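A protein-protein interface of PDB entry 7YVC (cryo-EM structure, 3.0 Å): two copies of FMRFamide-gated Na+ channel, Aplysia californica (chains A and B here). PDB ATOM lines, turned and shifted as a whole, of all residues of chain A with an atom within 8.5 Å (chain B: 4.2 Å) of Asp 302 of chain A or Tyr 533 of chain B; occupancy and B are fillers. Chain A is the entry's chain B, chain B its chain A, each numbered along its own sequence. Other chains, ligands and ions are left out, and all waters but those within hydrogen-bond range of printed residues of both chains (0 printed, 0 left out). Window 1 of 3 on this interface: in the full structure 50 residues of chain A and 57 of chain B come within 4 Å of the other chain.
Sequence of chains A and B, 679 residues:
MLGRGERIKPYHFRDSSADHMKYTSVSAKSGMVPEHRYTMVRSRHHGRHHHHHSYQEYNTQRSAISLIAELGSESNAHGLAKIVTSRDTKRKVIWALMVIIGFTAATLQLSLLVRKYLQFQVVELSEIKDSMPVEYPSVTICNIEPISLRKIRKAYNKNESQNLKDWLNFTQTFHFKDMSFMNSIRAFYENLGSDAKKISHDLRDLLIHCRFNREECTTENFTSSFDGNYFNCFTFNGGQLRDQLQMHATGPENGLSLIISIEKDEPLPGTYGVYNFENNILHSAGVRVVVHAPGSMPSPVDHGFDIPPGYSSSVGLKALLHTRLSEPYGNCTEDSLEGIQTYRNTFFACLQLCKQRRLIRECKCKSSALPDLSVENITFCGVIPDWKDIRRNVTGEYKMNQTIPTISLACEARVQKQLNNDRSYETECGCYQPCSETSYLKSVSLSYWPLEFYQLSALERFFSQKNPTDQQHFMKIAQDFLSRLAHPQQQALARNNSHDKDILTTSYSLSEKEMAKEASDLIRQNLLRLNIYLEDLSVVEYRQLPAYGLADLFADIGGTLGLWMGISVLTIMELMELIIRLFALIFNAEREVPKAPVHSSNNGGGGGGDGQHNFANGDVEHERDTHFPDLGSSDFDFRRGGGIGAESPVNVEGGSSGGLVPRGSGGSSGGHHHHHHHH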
ATOM      1  N   ASP A 227       7.140 -33.409  15.834  1.00  0.00           N
ATOM      2  CA  ASP A 227       5.864 -33.404  16.533  1.00  0.00           C
ATOM      3  C   ASP A 227       4.766 -33.956  15.639  1.00  0.00           C
ATOM      4  O   ASP A 227       4.833 -33.859  14.414  1.00  0.00           O
ATOM      5  CB  ASP A 227       5.476 -32.006  17.002  1.00  0.00           C
ATOM      6  CG  ASP A 227       4.507 -32.034  18.165  1.00  0.00           C
ATOM      7  OD1 ASP A 227       4.925 -32.417  19.276  1.00  0.00           O
ATOM      8  OD2 ASP A 227       3.328 -31.677  17.972  1.00  0.00           O
ATOM      9  N   ASN A 229       1.150 -33.648  14.021  1.00  0.00           N
ATOM     10  CA  ASN A 229       0.216 -32.625  13.543  1.00  0.00           C
ATOM     11  C   ASN A 229       0.796 -31.211  13.504  1.00  0.00           C
ATOM     12  O   ASN A 229       0.090 -30.272  13.130  1.00  0.00           O
ATOM     13  CB  ASN A 229      -1.104 -32.657  14.341  1.00  0.00           C
ATOM     14  CG  ASN A 229      -0.952 -32.260  15.792  1.00  0.00           C
ATOM     15  OD1 ASN A 229      -0.543 -31.149  16.105  1.00  0.00           O
ATOM     16  ND2 ASN A 229      -1.281 -33.178  16.689  1.00  0.00           N
ATOM     17  N   TYR A 230       2.072 -31.048  13.858  1.00  0.00           N
ATOM     18  CA  TYR A 230       2.830 -29.833  13.565  1.00  0.00           C
ATOM     19  C   TYR A 230       4.158 -30.127  12.895  1.00  0.00           C
ATOM     20  O   TYR A 230       4.709 -29.244  12.230  1.00  0.00           O
ATOM     21  CB  TYR A 230       3.094 -29.027  14.844  1.00  0.00           C
ATOM     22  CG  TYR A 230       1.849 -28.450  15.461  1.00  0.00           C
ATOM     23  CD1 TYR A 230       0.969 -27.699  14.709  1.00  0.00           C
ATOM     24  CD2 TYR A 230       1.549 -28.667  16.791  1.00  0.00           C
ATOM     25  CE1 TYR A 230      -0.171 -27.180  15.263  1.00  0.00           C
ATOM     26  CE2 TYR A 230       0.413 -28.153  17.351  1.00  0.00           C
ATOM     27  CZ  TYR A 230      -0.443 -27.409  16.582  1.00  0.00           C
ATOM     28  OH  TYR A 230      -1.584 -26.889  17.135  1.00  0.00           O
ATOM     29  N   ASN A 280      -9.903 -30.851  14.354  1.00  0.00           N
ATOM     30  CA  ASN A 280     -10.240 -29.580  14.976  1.00  0.00           C
ATOM     31  C   ASN A 280      -9.094 -28.580  14.966  1.00  0.00           C
ATOM     32  O   ASN A 280      -9.226 -27.509  15.559  1.00  0.00           O
ATOM     33  CB  ASN A 280     -10.694 -29.803  16.418  1.00  0.00           C
ATOM     34  CG  ASN A 280     -11.836 -30.774  16.524  1.00  0.00           C
ATOM     35  OD1 ASN A 280     -12.515 -31.055  15.544  1.00  0.00           O
ATOM     36  ND2 ASN A 280     -12.065 -31.287  17.720  1.00  0.00           N
ATOM     37  N   ILE A 281      -7.979 -28.894  14.315  1.00  0.00           N
ATOM     38  CA  ILE A 281      -6.775 -28.087  14.451  1.00  0.00           C
ATOM     39  C   ILE A 281      -6.302 -27.603  13.088  1.00  0.00           C
ATOM     40  O   ILE A 281      -5.645 -26.564  12.975  1.00  0.00           O
ATOM     41  CB  ILE A 281      -5.677 -28.893  15.165  1.00  0.00           C
ATOM     42  CG1 ILE A 281      -6.092 -29.179  16.598  1.00  0.00           C
ATOM     43  CG2 ILE A 281      -4.358 -28.155  15.177  1.00  0.00           C
ATOM     44  CD1 ILE A 281      -5.129 -30.062  17.299  1.00  0.00           C
ATOM     45  N   ARG A 288       2.147 -21.864  17.093  1.00  0.00           N
ATOM     46  CA  ARG A 288       1.794 -22.481  18.363  1.00  0.00           C
ATOM     47  C   ARG A 288       2.974 -22.356  19.316  1.00  0.00           C
ATOM     48  O   ARG A 288       4.059 -22.869  19.030  1.00  0.00           O
ATOM     49  CB  ARG A 288       1.421 -23.946  18.166  1.00  0.00           C
ATOM     50  CG  ARG A 288       0.758 -24.574  19.359  1.00  0.00           C
ATOM     51  CD  ARG A 288      -0.736 -24.510  19.226  1.00  0.00           C
ATOM     52  NE  ARG A 288      -1.412 -25.033  20.403  1.00  0.00           N
ATOM     53  CZ  ARG A 288      -2.720 -24.944  20.606  1.00  0.00           C
ATOM     54  NH1 ARG A 288      -3.488 -24.351  19.706  1.00  0.00           N
ATOM     55  NH2 ARG A 288      -3.260 -25.446  21.703  1.00  0.00           N
ATOM     56  N   VAL A 289       2.767 -21.683  20.442  1.00  0.00           N
ATOM     57  CA  VAL A 289       3.828 -21.380  21.390  1.00  0.00           C
ATOM     58  C   VAL A 289       3.551 -22.127  22.682  1.00  0.00           C
ATOM     59  O   VAL A 289       2.415 -22.141  23.164  1.00  0.00           O
ATOM     60  CB  VAL A 289       3.935 -19.870  21.648  1.00  0.00           C
ATOM     61  CG1 VAL A 289       5.154 -19.565  22.477  1.00  0.00           C
ATOM     62  CG2 VAL A 289       3.986 -19.124  20.344  1.00  0.00           C
ATOM     63  N   VAL A 290       4.582 -22.758  23.232  1.00  0.00           N
ATOM     64  CA  VAL A 290       4.516 -23.425  24.524  1.00  0.00           C
ATOM     65  C   VAL A 290       5.583 -22.808  25.407  1.00  0.00           C
ATOM     66  O   VAL A 290       6.758 -22.762  25.028  1.00  0.00           O
ATOM     67  CB  VAL A 290       4.728 -24.940  24.404  1.00  0.00           C
ATOM     68  CG1 VAL A 290       4.380 -25.619  25.702  1.00  0.00           C
ATOM     69  CG2 VAL A 290       3.908 -25.492  23.286  1.00  0.00           C
ATOM     70  N   PRO A 298       7.935 -30.594  26.093  1.00  0.00           N
ATOM     71  CA  PRO A 298       6.843 -29.795  25.534  1.00  0.00           C
ATOM     72  C   PRO A 298       5.653 -30.657  25.148  1.00  0.00           C
ATOM     73  O   PRO A 298       5.760 -31.869  24.954  1.00  0.00           O
ATOM     74  CB  PRO A 298       7.476 -29.150  24.300  1.00  0.00           C
ATOM     75  CG  PRO A 298       8.532 -30.095  23.899  1.00  0.00           C
ATOM     76  CD  PRO A 298       9.060 -30.721  25.155  1.00  0.00           C
ATOM     77  N   SER A 299       4.500 -30.004  25.034  1.00  0.00           N
ATOM     78  CA  SER A 299       3.277 -30.634  24.536  1.00  0.00           C
ATOM     79  C   SER A 299       2.491 -29.591  23.761  1.00  0.00           C
ATOM     80  O   SER A 299       1.531 -29.006  24.273  1.00  0.00           O
ATOM     81  CB  SER A 299       2.447 -31.214  25.679  1.00  0.00           C
ATOM     82  OG  SER A 299       3.172 -32.209  26.373  1.00  0.00           O
ATOM     83  N   PRO A 300       2.878 -29.330  22.512  1.00  0.00           N
ATOM     84  CA  PRO A 300       2.282 -28.200  21.783  1.00  0.00           C
ATOM     85  C   PRO A 300       0.780 -28.292  21.596  1.00  0.00           C
ATOM     86  O   PRO A 300       0.102 -27.261  21.608  1.00  0.00           O
ATOM     87  CB  PRO A 300       3.020 -28.237  20.440  1.00  0.00           C
ATOM     88  CG  PRO A 300       4.263 -28.969  20.713  1.00  0.00           C
ATOM     89  CD  PRO A 300       3.929 -29.990  21.730  1.00  0.00           C
ATOM     90  N   VAL A 301       0.237 -29.493  21.409  1.00  0.00           N
ATOM     91  CA  VAL A 301      -1.189 -29.613  21.136  1.00  0.00           C
ATOM     92  C   VAL A 301      -2.004 -29.298  22.384  1.00  0.00           C
ATOM     93  O   VAL A 301      -3.044 -28.636  22.311  1.00  0.00           O
ATOM     94  CB  VAL A 301      -1.507 -31.012  20.582  1.00  0.00           C
ATOM     95  CG1 VAL A 301      -2.970 -31.127  20.244  1.00  0.00           C
ATOM     96  CG2 VAL A 301      -0.668 -31.291  19.362  1.00  0.00           C
ATOM     97  N   ASP A 302      -1.545 -29.753  23.544  1.00  0.00           N
ATOM     98  CA  ASP A 302      -2.302 -29.598  24.779  1.00  0.00           C
ATOM     99  C   ASP A 302      -2.055 -28.254  25.456  1.00  0.00           C
ATOM    100  O   ASP A 302      -3.005 -27.541  25.789  1.00  0.00           O
ATOM    101  CB  ASP A 302      -1.951 -30.728  25.743  1.00  0.00           C
ATOM    102  CG  ASP A 302      -2.342 -32.081  25.214  1.00  0.00           C
ATOM    103  OD1 ASP A 302      -3.517 -32.455  25.371  1.00  0.00           O
ATOM    104  OD2 ASP A 302      -1.480 -32.771  24.636  1.00  0.00           O
ATOM    105  N   HIS A 303      -0.791 -27.898  25.670  1.00  0.00           N
ATOM    106  CA  HIS A 303      -0.434 -26.757  26.498  1.00  0.00           C
ATOM    107  C   HIS A 303      -0.035 -25.522  25.705  1.00  0.00           C
ATOM    108  O   HIS A 303       0.348 -24.519  26.309  1.00  0.00           O
ATOM    109  CB  HIS A 303       0.703 -27.140  27.442  1.00  0.00           C
ATOM    110  CG  HIS A 303       0.350 -28.233  28.399  1.00  0.00           C
ATOM    111  ND1 HIS A 303       0.317 -29.560  28.034  1.00  0.00           N
ATOM    112  CD2 HIS A 303       0.017 -28.196  29.709  1.00  0.00           C
ATOM    113  CE1 HIS A 303      -0.022 -30.293  29.077  1.00  0.00           C
ATOM    114  NE2 HIS A 303      -0.210 -29.490  30.107  1.00  0.00           N
ATOM    115  N   GLY A 304      -0.106 -25.559  24.388  1.00  0.00           N
ATOM    116  CA  GLY A 304       0.274 -24.405  23.607  1.00  0.00           C
ATOM    117  C   GLY A 304      -0.819 -23.363  23.527  1.00  0.00           C
ATOM    118  O   GLY A 304      -1.937 -23.554  23.996  1.00  0.00           O
ATOM    119  N   PHE A 305      -0.473 -22.224  22.934  1.00  0.00           N
ATOM    120  CA  PHE A 305      -1.450 -21.209  22.578  1.00  0.00           C
ATOM    121  C   PHE A 305      -1.071 -20.630  21.226  1.00  0.00           C
ATOM    122  O   PHE A 305       0.105 -20.577  20.868  1.00  0.00           O
ATOM    123  CB  PHE A 305      -1.562 -20.111  23.648  1.00  0.00           C
ATOM    124  CG  PHE A 305      -0.281 -19.385  23.928  1.00  0.00           C
ATOM    125  CD1 PHE A 305       0.601 -19.856  24.874  1.00  0.00           C
ATOM    126  CD2 PHE A 305       0.024 -18.214  23.266  1.00  0.00           C
ATOM    127  CE1 PHE A 305       1.767 -19.188  25.135  1.00  0.00           C
ATOM    128  CE2 PHE A 305       1.190 -17.549  23.526  1.00  0.00           C
ATOM    129  CZ  PHE A 305       2.061 -18.036  24.460  1.00  0.00           C
ATOM    130  N   ASP A 306      -2.077 -20.216  20.468  1.00  0.00           N
ATOM    131  CA  ASP A 306      -1.862 -19.773  19.101  1.00  0.00           C
ATOM    132  C   ASP A 306      -1.547 -18.286  19.053  1.00  0.00           C
ATOM    133  O   ASP A 306      -1.967 -17.510  19.910  1.00  0.00           O
ATOM    134  CB  ASP A 306      -3.086 -20.051  18.232  1.00  0.00           C
ATOM    135  CG  ASP A 306      -3.616 -21.456  18.386  1.00  0.00           C
ATOM    136  OD1 ASP A 306      -2.872 -22.415  18.101  1.00  0.00           O
ATOM    137  OD2 ASP A 306      -4.795 -21.606  18.769  1.00  0.00           O
ATOM    138  N   PHE A 348       2.365 -34.837  33.329  1.00  0.00           N
ATOM    139  CA  PHE A 348       1.734 -35.057  32.031  1.00  0.00           C
ATOM    140  C   PHE A 348       2.659 -35.816  31.089  1.00  0.00           C
ATOM    141  O   PHE A 348       2.223 -36.725  30.371  1.00  0.00           O
ATOM    142  CB  PHE A 348       1.325 -33.713  31.432  1.00  0.00           C
ATOM    143  CG  PHE A 348       0.610 -33.822  30.122  1.00  0.00           C
ATOM    144  CD1 PHE A 348      -0.736 -34.110  30.076  1.00  0.00           C
ATOM    145  CD2 PHE A 348       1.283 -33.614  28.937  1.00  0.00           C
ATOM    146  CE1 PHE A 348      -1.393 -34.203  28.874  1.00  0.00           C
ATOM    147  CE2 PHE A 348       0.630 -33.706  27.734  1.00  0.00           C
ATOM    148  CZ  PHE A 348      -0.708 -34.001  27.702  1.00  0.00           C
ATOM    149  N   GLN A 352       2.241 -39.471  29.205  1.00  0.00           N
ATOM    150  CA  GLN A 352       2.433 -39.714  27.776  1.00  0.00           C
ATOM    151  C   GLN A 352       3.421 -40.852  27.533  1.00  0.00           C
ATOM    152  O   GLN A 352       3.195 -41.715  26.672  1.00  0.00           O
ATOM    153  CB  GLN A 352       2.901 -38.439  27.084  1.00  0.00           C
ATOM    154  CG  GLN A 352       1.975 -37.260  27.264  1.00  0.00           C
ATOM    155  CD  GLN A 352       0.595 -37.512  26.711  1.00  0.00           C
ATOM    156  OE1 GLN A 352       0.376 -37.445  25.506  1.00  0.00           O
ATOM    157  NE2 GLN A 352      -0.350 -37.799  27.593  1.00  0.00           N
ATOM    158  N   LYS A 355       1.693 -44.084  28.175  1.00  0.00           N
ATOM    159  CA  LYS A 355       0.889 -44.488  27.027  1.00  0.00           C
ATOM    160  C   LYS A 355       1.756 -45.145  25.961  1.00  0.00           C
ATOM    161  O   LYS A 355       1.391 -46.183  25.392  1.00  0.00           O
ATOM    162  CB  LYS A 355       0.177 -43.275  26.438  1.00  0.00           C
ATOM    163  CG  LYS A 355      -1.101 -42.868  27.121  1.00  0.00           C
ATOM    164  CD  LYS A 355      -1.602 -41.585  26.498  1.00  0.00           C
ATOM    165  CE  LYS A 355      -3.052 -41.333  26.808  1.00  0.00           C
ATOM    166  NZ  LYS A 355      -3.492 -40.025  26.265  1.00  0.00           N
ATOM    167  N   ALA A 369       1.990 -40.034  17.315  1.00  0.00           N
ATOM    168  CA  ALA A 369       1.265 -39.027  18.074  1.00  0.00           C
ATOM    169  C   ALA A 369       1.604 -39.046  19.554  1.00  0.00           C
ATOM    170  O   ALA A 369       0.883 -38.437  20.348  1.00  0.00           O
ATOM    171  CB  ALA A 369      -0.241 -39.217  17.887  1.00  0.00           C
ATOM    172  N   THR B 250      -7.223 -35.047  26.835  1.00  0.00           N
ATOM    173  CA  THR B 250      -6.869 -33.640  26.775  1.00  0.00           C
ATOM    174  C   THR B 250      -6.589 -33.237  25.337  1.00  0.00           C
ATOM    175  O   THR B 250      -6.405 -34.081  24.458  1.00  0.00           O
ATOM    176  CB  THR B 250      -5.641 -33.338  27.636  1.00  0.00           C
ATOM    177  OG1 THR B 250      -4.515 -34.047  27.111  1.00  0.00           O
ATOM    178  CG2 THR B 250      -5.871 -33.766  29.061  1.00  0.00           C
ATOM    179  N   GLY B 251      -6.555 -31.933  25.101  1.00  0.00           N
ATOM    180  CA  GLY B 251      -6.199 -31.415  23.806  1.00  0.00           C
ATOM    181  C   GLY B 251      -7.400 -31.069  22.959  1.00  0.00           C
ATOM    182  O   GLY B 251      -8.529 -31.468  23.244  1.00  0.00           O
ATOM    183  N   PRO B 252      -7.169 -30.300  21.898  1.00  0.00           N
ATOM    184  CA  PRO B 252      -8.284 -29.858  21.051  1.00  0.00           C
ATOM    185  C   PRO B 252      -9.033 -30.977  20.355  1.00  0.00           C
ATOM    186  O   PRO B 252     -10.214 -30.794  20.038  1.00  0.00           O
ATOM    187  CB  PRO B 252      -7.599 -28.932  20.038  1.00  0.00           C
ATOM    188  CG  PRO B 252      -6.343 -28.523  20.681  1.00  0.00           C
ATOM    189  CD  PRO B 252      -5.904 -29.662  21.522  1.00  0.00           C
ATOM    190  N   GLY B 255     -11.947 -32.380  22.779  1.00  0.00           N
ATOM    191  CA  GLY B 255     -12.892 -31.455  23.360  1.00  0.00           C
ATOM    192  C   GLY B 255     -13.990 -31.074  22.390  1.00  0.00           C
ATOM    193  O   GLY B 255     -14.182 -31.689  21.341  1.00  0.00           O
ATOM    194  N   SER B 314      -9.063 -20.907  20.486  1.00  0.00           N
ATOM    195  CA  SER B 314      -8.994 -22.085  21.332  1.00  0.00           C
ATOM    196  C   SER B 314      -8.981 -21.656  22.787  1.00  0.00           C
ATOM    197  O   SER B 314      -8.258 -20.724  23.158  1.00  0.00           O
ATOM    198  CB  SER B 314      -7.759 -22.923  21.009  1.00  0.00           C
ATOM    199  OG  SER B 314      -6.579 -22.152  21.096  1.00  0.00           O
ATOM    200  N   VAL B 315      -9.791 -22.328  23.598  1.00  0.00           N
ATOM    201  CA  VAL B 315      -9.909 -22.065  25.022  1.00  0.00           C
ATOM    202  C   VAL B 315      -9.450 -23.319  25.743  1.00  0.00           C
ATOM    203  O   VAL B 315     -10.108 -24.360  25.662  1.00  0.00           O
ATOM    204  CB  VAL B 315     -11.345 -21.703  25.419  1.00  0.00           C
ATOM    205  CG1 VAL B 315     -11.403 -21.277  26.863  1.00  0.00           C
ATOM    206  CG2 VAL B 315     -11.877 -20.616  24.525  1.00  0.00           C
ATOM    207  N   GLY B 316      -8.327 -23.227  26.448  1.00  0.00           N
ATOM    208  CA  GLY B 316      -7.812 -24.337  27.225  1.00  0.00           C
ATOM    209  C   GLY B 316      -8.162 -24.148  28.689  1.00  0.00           C
ATOM    210  O   GLY B 316      -7.904 -23.093  29.264  1.00  0.00           O
ATOM    211  N   LEU B 317      -8.749 -25.183  29.280  1.00  0.00           N
ATOM    212  CA  LEU B 317      -9.315 -25.107  30.617  1.00  0.00           C
ATOM    213  C   LEU B 317      -8.542 -25.978  31.593  1.00  0.00           C
ATOM    214  O   LEU B 317      -8.083 -27.067  31.243  1.00  0.00           O
ATOM    215  CB  LEU B 317     -10.778 -25.543  30.616  1.00  0.00           C
ATOM    216  CG  LEU B 317     -11.729 -24.793  29.699  1.00  0.00           C
ATOM    217  CD1 LEU B 317     -12.962 -25.623  29.485  1.00  0.00           C
ATOM    218  CD2 LEU B 317     -12.077 -23.466  30.309  1.00  0.00           C
ATOM    219  N   ASN B 531     -12.692 -23.986  19.751  1.00  0.00           N
ATOM    220  CA  ASN B 531     -12.337 -25.246  20.388  1.00  0.00           C
ATOM    221  C   ASN B 531     -12.230 -25.011  21.883  1.00  0.00           C
ATOM    222  O   ASN B 531     -11.452 -24.163  22.322  1.00  0.00           O
ATOM    223  CB  ASN B 531     -11.017 -25.792  19.852  1.00  0.00           C
ATOM    224  CG  ASN B 531     -11.028 -25.987  18.364  1.00  0.00           C
ATOM    225  OD1 ASN B 531     -12.026 -26.404  17.789  1.00  0.00           O
ATOM    226  ND2 ASN B 531      -9.913 -25.690  17.726  1.00  0.00           N
ATOM    227  N   ILE B 532     -13.000 -25.762  22.658  1.00  0.00           N
ATOM    228  CA  ILE B 532     -12.960 -25.702  24.112  1.00  0.00           C
ATOM    229  C   ILE B 532     -12.556 -27.077  24.607  1.00  0.00           C
ATOM    230  O   ILE B 532     -13.241 -28.066  24.325  1.00  0.00           O
ATOM    231  CB  ILE B 532     -14.308 -25.269  24.700  1.00  0.00           C
ATOM    232  CG1 ILE B 532     -14.753 -23.961  24.060  1.00  0.00           C
ATOM    233  CG2 ILE B 532     -14.202 -25.087  26.181  1.00  0.00           C
ATOM    234  CD1 ILE B 532     -16.151 -23.583  24.377  1.00  0.00           C
ATOM    235  N   TYR B 533     -11.450 -27.146  25.339  1.00  0.00           N
ATOM    236  CA  TYR B 533     -10.874 -28.427  25.708  1.00  0.00           C
ATOM    237  C   TYR B 533     -10.220 -28.311  27.073  1.00  0.00           C
ATOM    238  O   TYR B 533     -10.014 -27.217  27.595  1.00  0.00           O
ATOM    239  CB  TYR B 533      -9.865 -28.898  24.663  1.00  0.00           C
ATOM    240  CG  TYR B 533      -8.754 -27.916  24.379  1.00  0.00           C
ATOM    241  CD1 TYR B 533      -7.601 -27.904  25.143  1.00  0.00           C
ATOM    242  CD2 TYR B 533      -8.851 -27.014  23.337  1.00  0.00           C
ATOM    243  CE1 TYR B 533      -6.591 -27.019  24.885  1.00  0.00           C
ATOM    244  CE2 TYR B 533      -7.842 -26.126  23.074  1.00  0.00           C
ATOM    245  CZ  TYR B 533      -6.716 -26.133  23.851  1.00  0.00           C
ATOM    246  OH  TYR B 533      -5.703 -25.250  23.594  1.00  0.00           O
ATOM    247  N   LEU B 534      -9.891 -29.462  27.646  1.00  0.00           N
ATOM    248  CA  LEU B 534      -9.236 -29.534  28.944  1.00  0.00           C
ATOM    249  C   LEU B 534      -7.732 -29.639  28.729  1.00  0.00           C
ATOM    250  O   LEU B 534      -7.268 -30.524  28.007  1.00  0.00           O
ATOM    251  CB  LEU B 534      -9.749 -30.731  29.741  1.00  0.00           C
ATOM    252  CG  LEU B 534     -10.926 -30.567  30.708  1.00  0.00           C
ATOM    253  CD1 LEU B 534     -10.542 -29.738  31.912  1.00  0.00           C
ATOM    254  CD2 LEU B 534     -12.121 -29.964  30.018  1.00  0.00           C
ATOM    255  N   GLU B 535      -6.971 -28.736  29.346  1.00  0.00           N
ATOM    256  CA  GLU B 535      -5.523 -28.762  29.171  1.00  0.00           C
ATOM    257  C   GLU B 535      -4.893 -29.903  29.953  1.00  0.00           C
ATOM    258  O   GLU B 535      -3.975 -30.568  29.465  1.00  0.00           O
ATOM    259  CB  GLU B 535      -4.916 -27.431  29.600  1.00  0.00           C
ATOM    260  CG  GLU B 535      -4.778 -26.428  28.484  1.00  0.00           C
ATOM    261  CD  GLU B 535      -4.010 -25.199  28.909  1.00  0.00           C
ATOM    262  OE1 GLU B 535      -3.748 -25.058  30.118  1.00  0.00           O
ATOM    263  OE2 GLU B 535      -3.670 -24.370  28.037  1.00  0.00           O
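OG1 of Thr 250 of chain B sits at hydrogen-bond distance from OD1 of Asp 302 of chain A (2.6 Å).
N of Gly 251 of chain B lies within hydrogen-bond range of OD1 of Asp 302 of chain A (3.1 Å).
The backbone carbonyl oxygen (O) of Pro 252 of chain B is in hydrogen-bond range of the side-chain amide nitrogen (ND2) of Asn 280 of chain A (3.0 Å).
The side-chain carboxylate (OD2) of Asp 306 of chain A is in hydrogen-bond range of the side-chain hydroxyl (OG) of Ser 314 of chain B, at 3.0 Å.
ND2 of Asn 531 of chain B lies within hydrogen-bond range of O of Asn 280 of chain A, at 2.9 Å.
NH2 of Arg 288 of chain A lies within hydrogen-bond range of OH of Tyr 533 of chain B, at 3.1 Å.
The backbone NH (N) of Gly 251 of chain B sits at hydrogen-bond distance from the backbone carbonyl oxygen (O) of Leu 534 of chain B (3.3 Å).
N of Tyr 533 of chain B lies within hydrogen-bond range of O of Val 315 of chain B, at 3.1 Å.
The backbone NH (N) of Leu 317 of chain B sits at hydrogen-bond distance from the backbone carbonyl oxygen (O) of Tyr 533 of chain B (2.9 Å).
NE of Arg 288 of chain A sits at hydrogen-bond distance from O of Pro 300 of chain A.
The guanidinium group (NH2) of Arg 288 of chain A sits at hydrogen-bond distance from the backbone carbonyl oxygen (O) of Val 301 of chain A (3.3 Å).
The backbone carbonyl oxygen of Gly 304 of chain A lies within hydrogen-bond range of the guanidinium group of Arg 288 of chain A (3.3 Å).
Among the printed residues, merely in contact across the chains: Val 301 of chain A with Pro 252 of chain B (3.1 Å), Asp 302 of chain A with Glu 535 of chain B (3.4 Å), Phe 348 of chain A with Thr 250 of chain B (3.6 Å), Asp 302 of chain A with Tyr 533 of chain B (3.7 Å), Ile 281 of chain A with Pro 252 of chain B (3.8 Å) and His 303 of chain A with Glu 535 of chain B (3.97 Å).
Tyr 533 of chain B touches just these residues of chain A: Arg 288 (3.1 Å) and Asp 302 (3.7 Å).
Of the printed residues of chain A, Pro 252 of chain B touches Asn 280 (3.0 Å), Ile 281 (3.8 Å) and Val 301 (3.1 Å).
Of the printed residues of chain B, Asn 280 of chain A touches Pro 252 and Asn 531.
Of the printed residues of chain A, Glu 535 of chain B touches Asp 302 (3.4 Å) and His 303 (3.97 Å).
The nearest printed residue of chain B that does not touch His 303 of chain A is Tyr 533 of chain B (5.9 Å).
Of the 21 printed residues of chain A, 8 touch a printed residue of chain B.
Hydrophobic or aromatic side chains of chain A that line the printed part of chain B: Ile 281, Val 301, His 303 and Phe 348.
Printed residues of chain B that touch a printed residue of chain A: Thr 250, Gly 251, Pro 252, Ser 314, Asn 531, Tyr 533 and Glu 535.
Along chain B the printed residues that touch a printed residue of chain A span positions 250 to 535.
Among the printed residues, no Asp or Glu carboxylate lies within 4 Å of a Lys or Arg side-chain nitrogen of the other chain.
No position is printed for both chains.
Of the 12 pairs that touch across the chains among the printed residues, none has its exchanged pair printed and touching as well.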
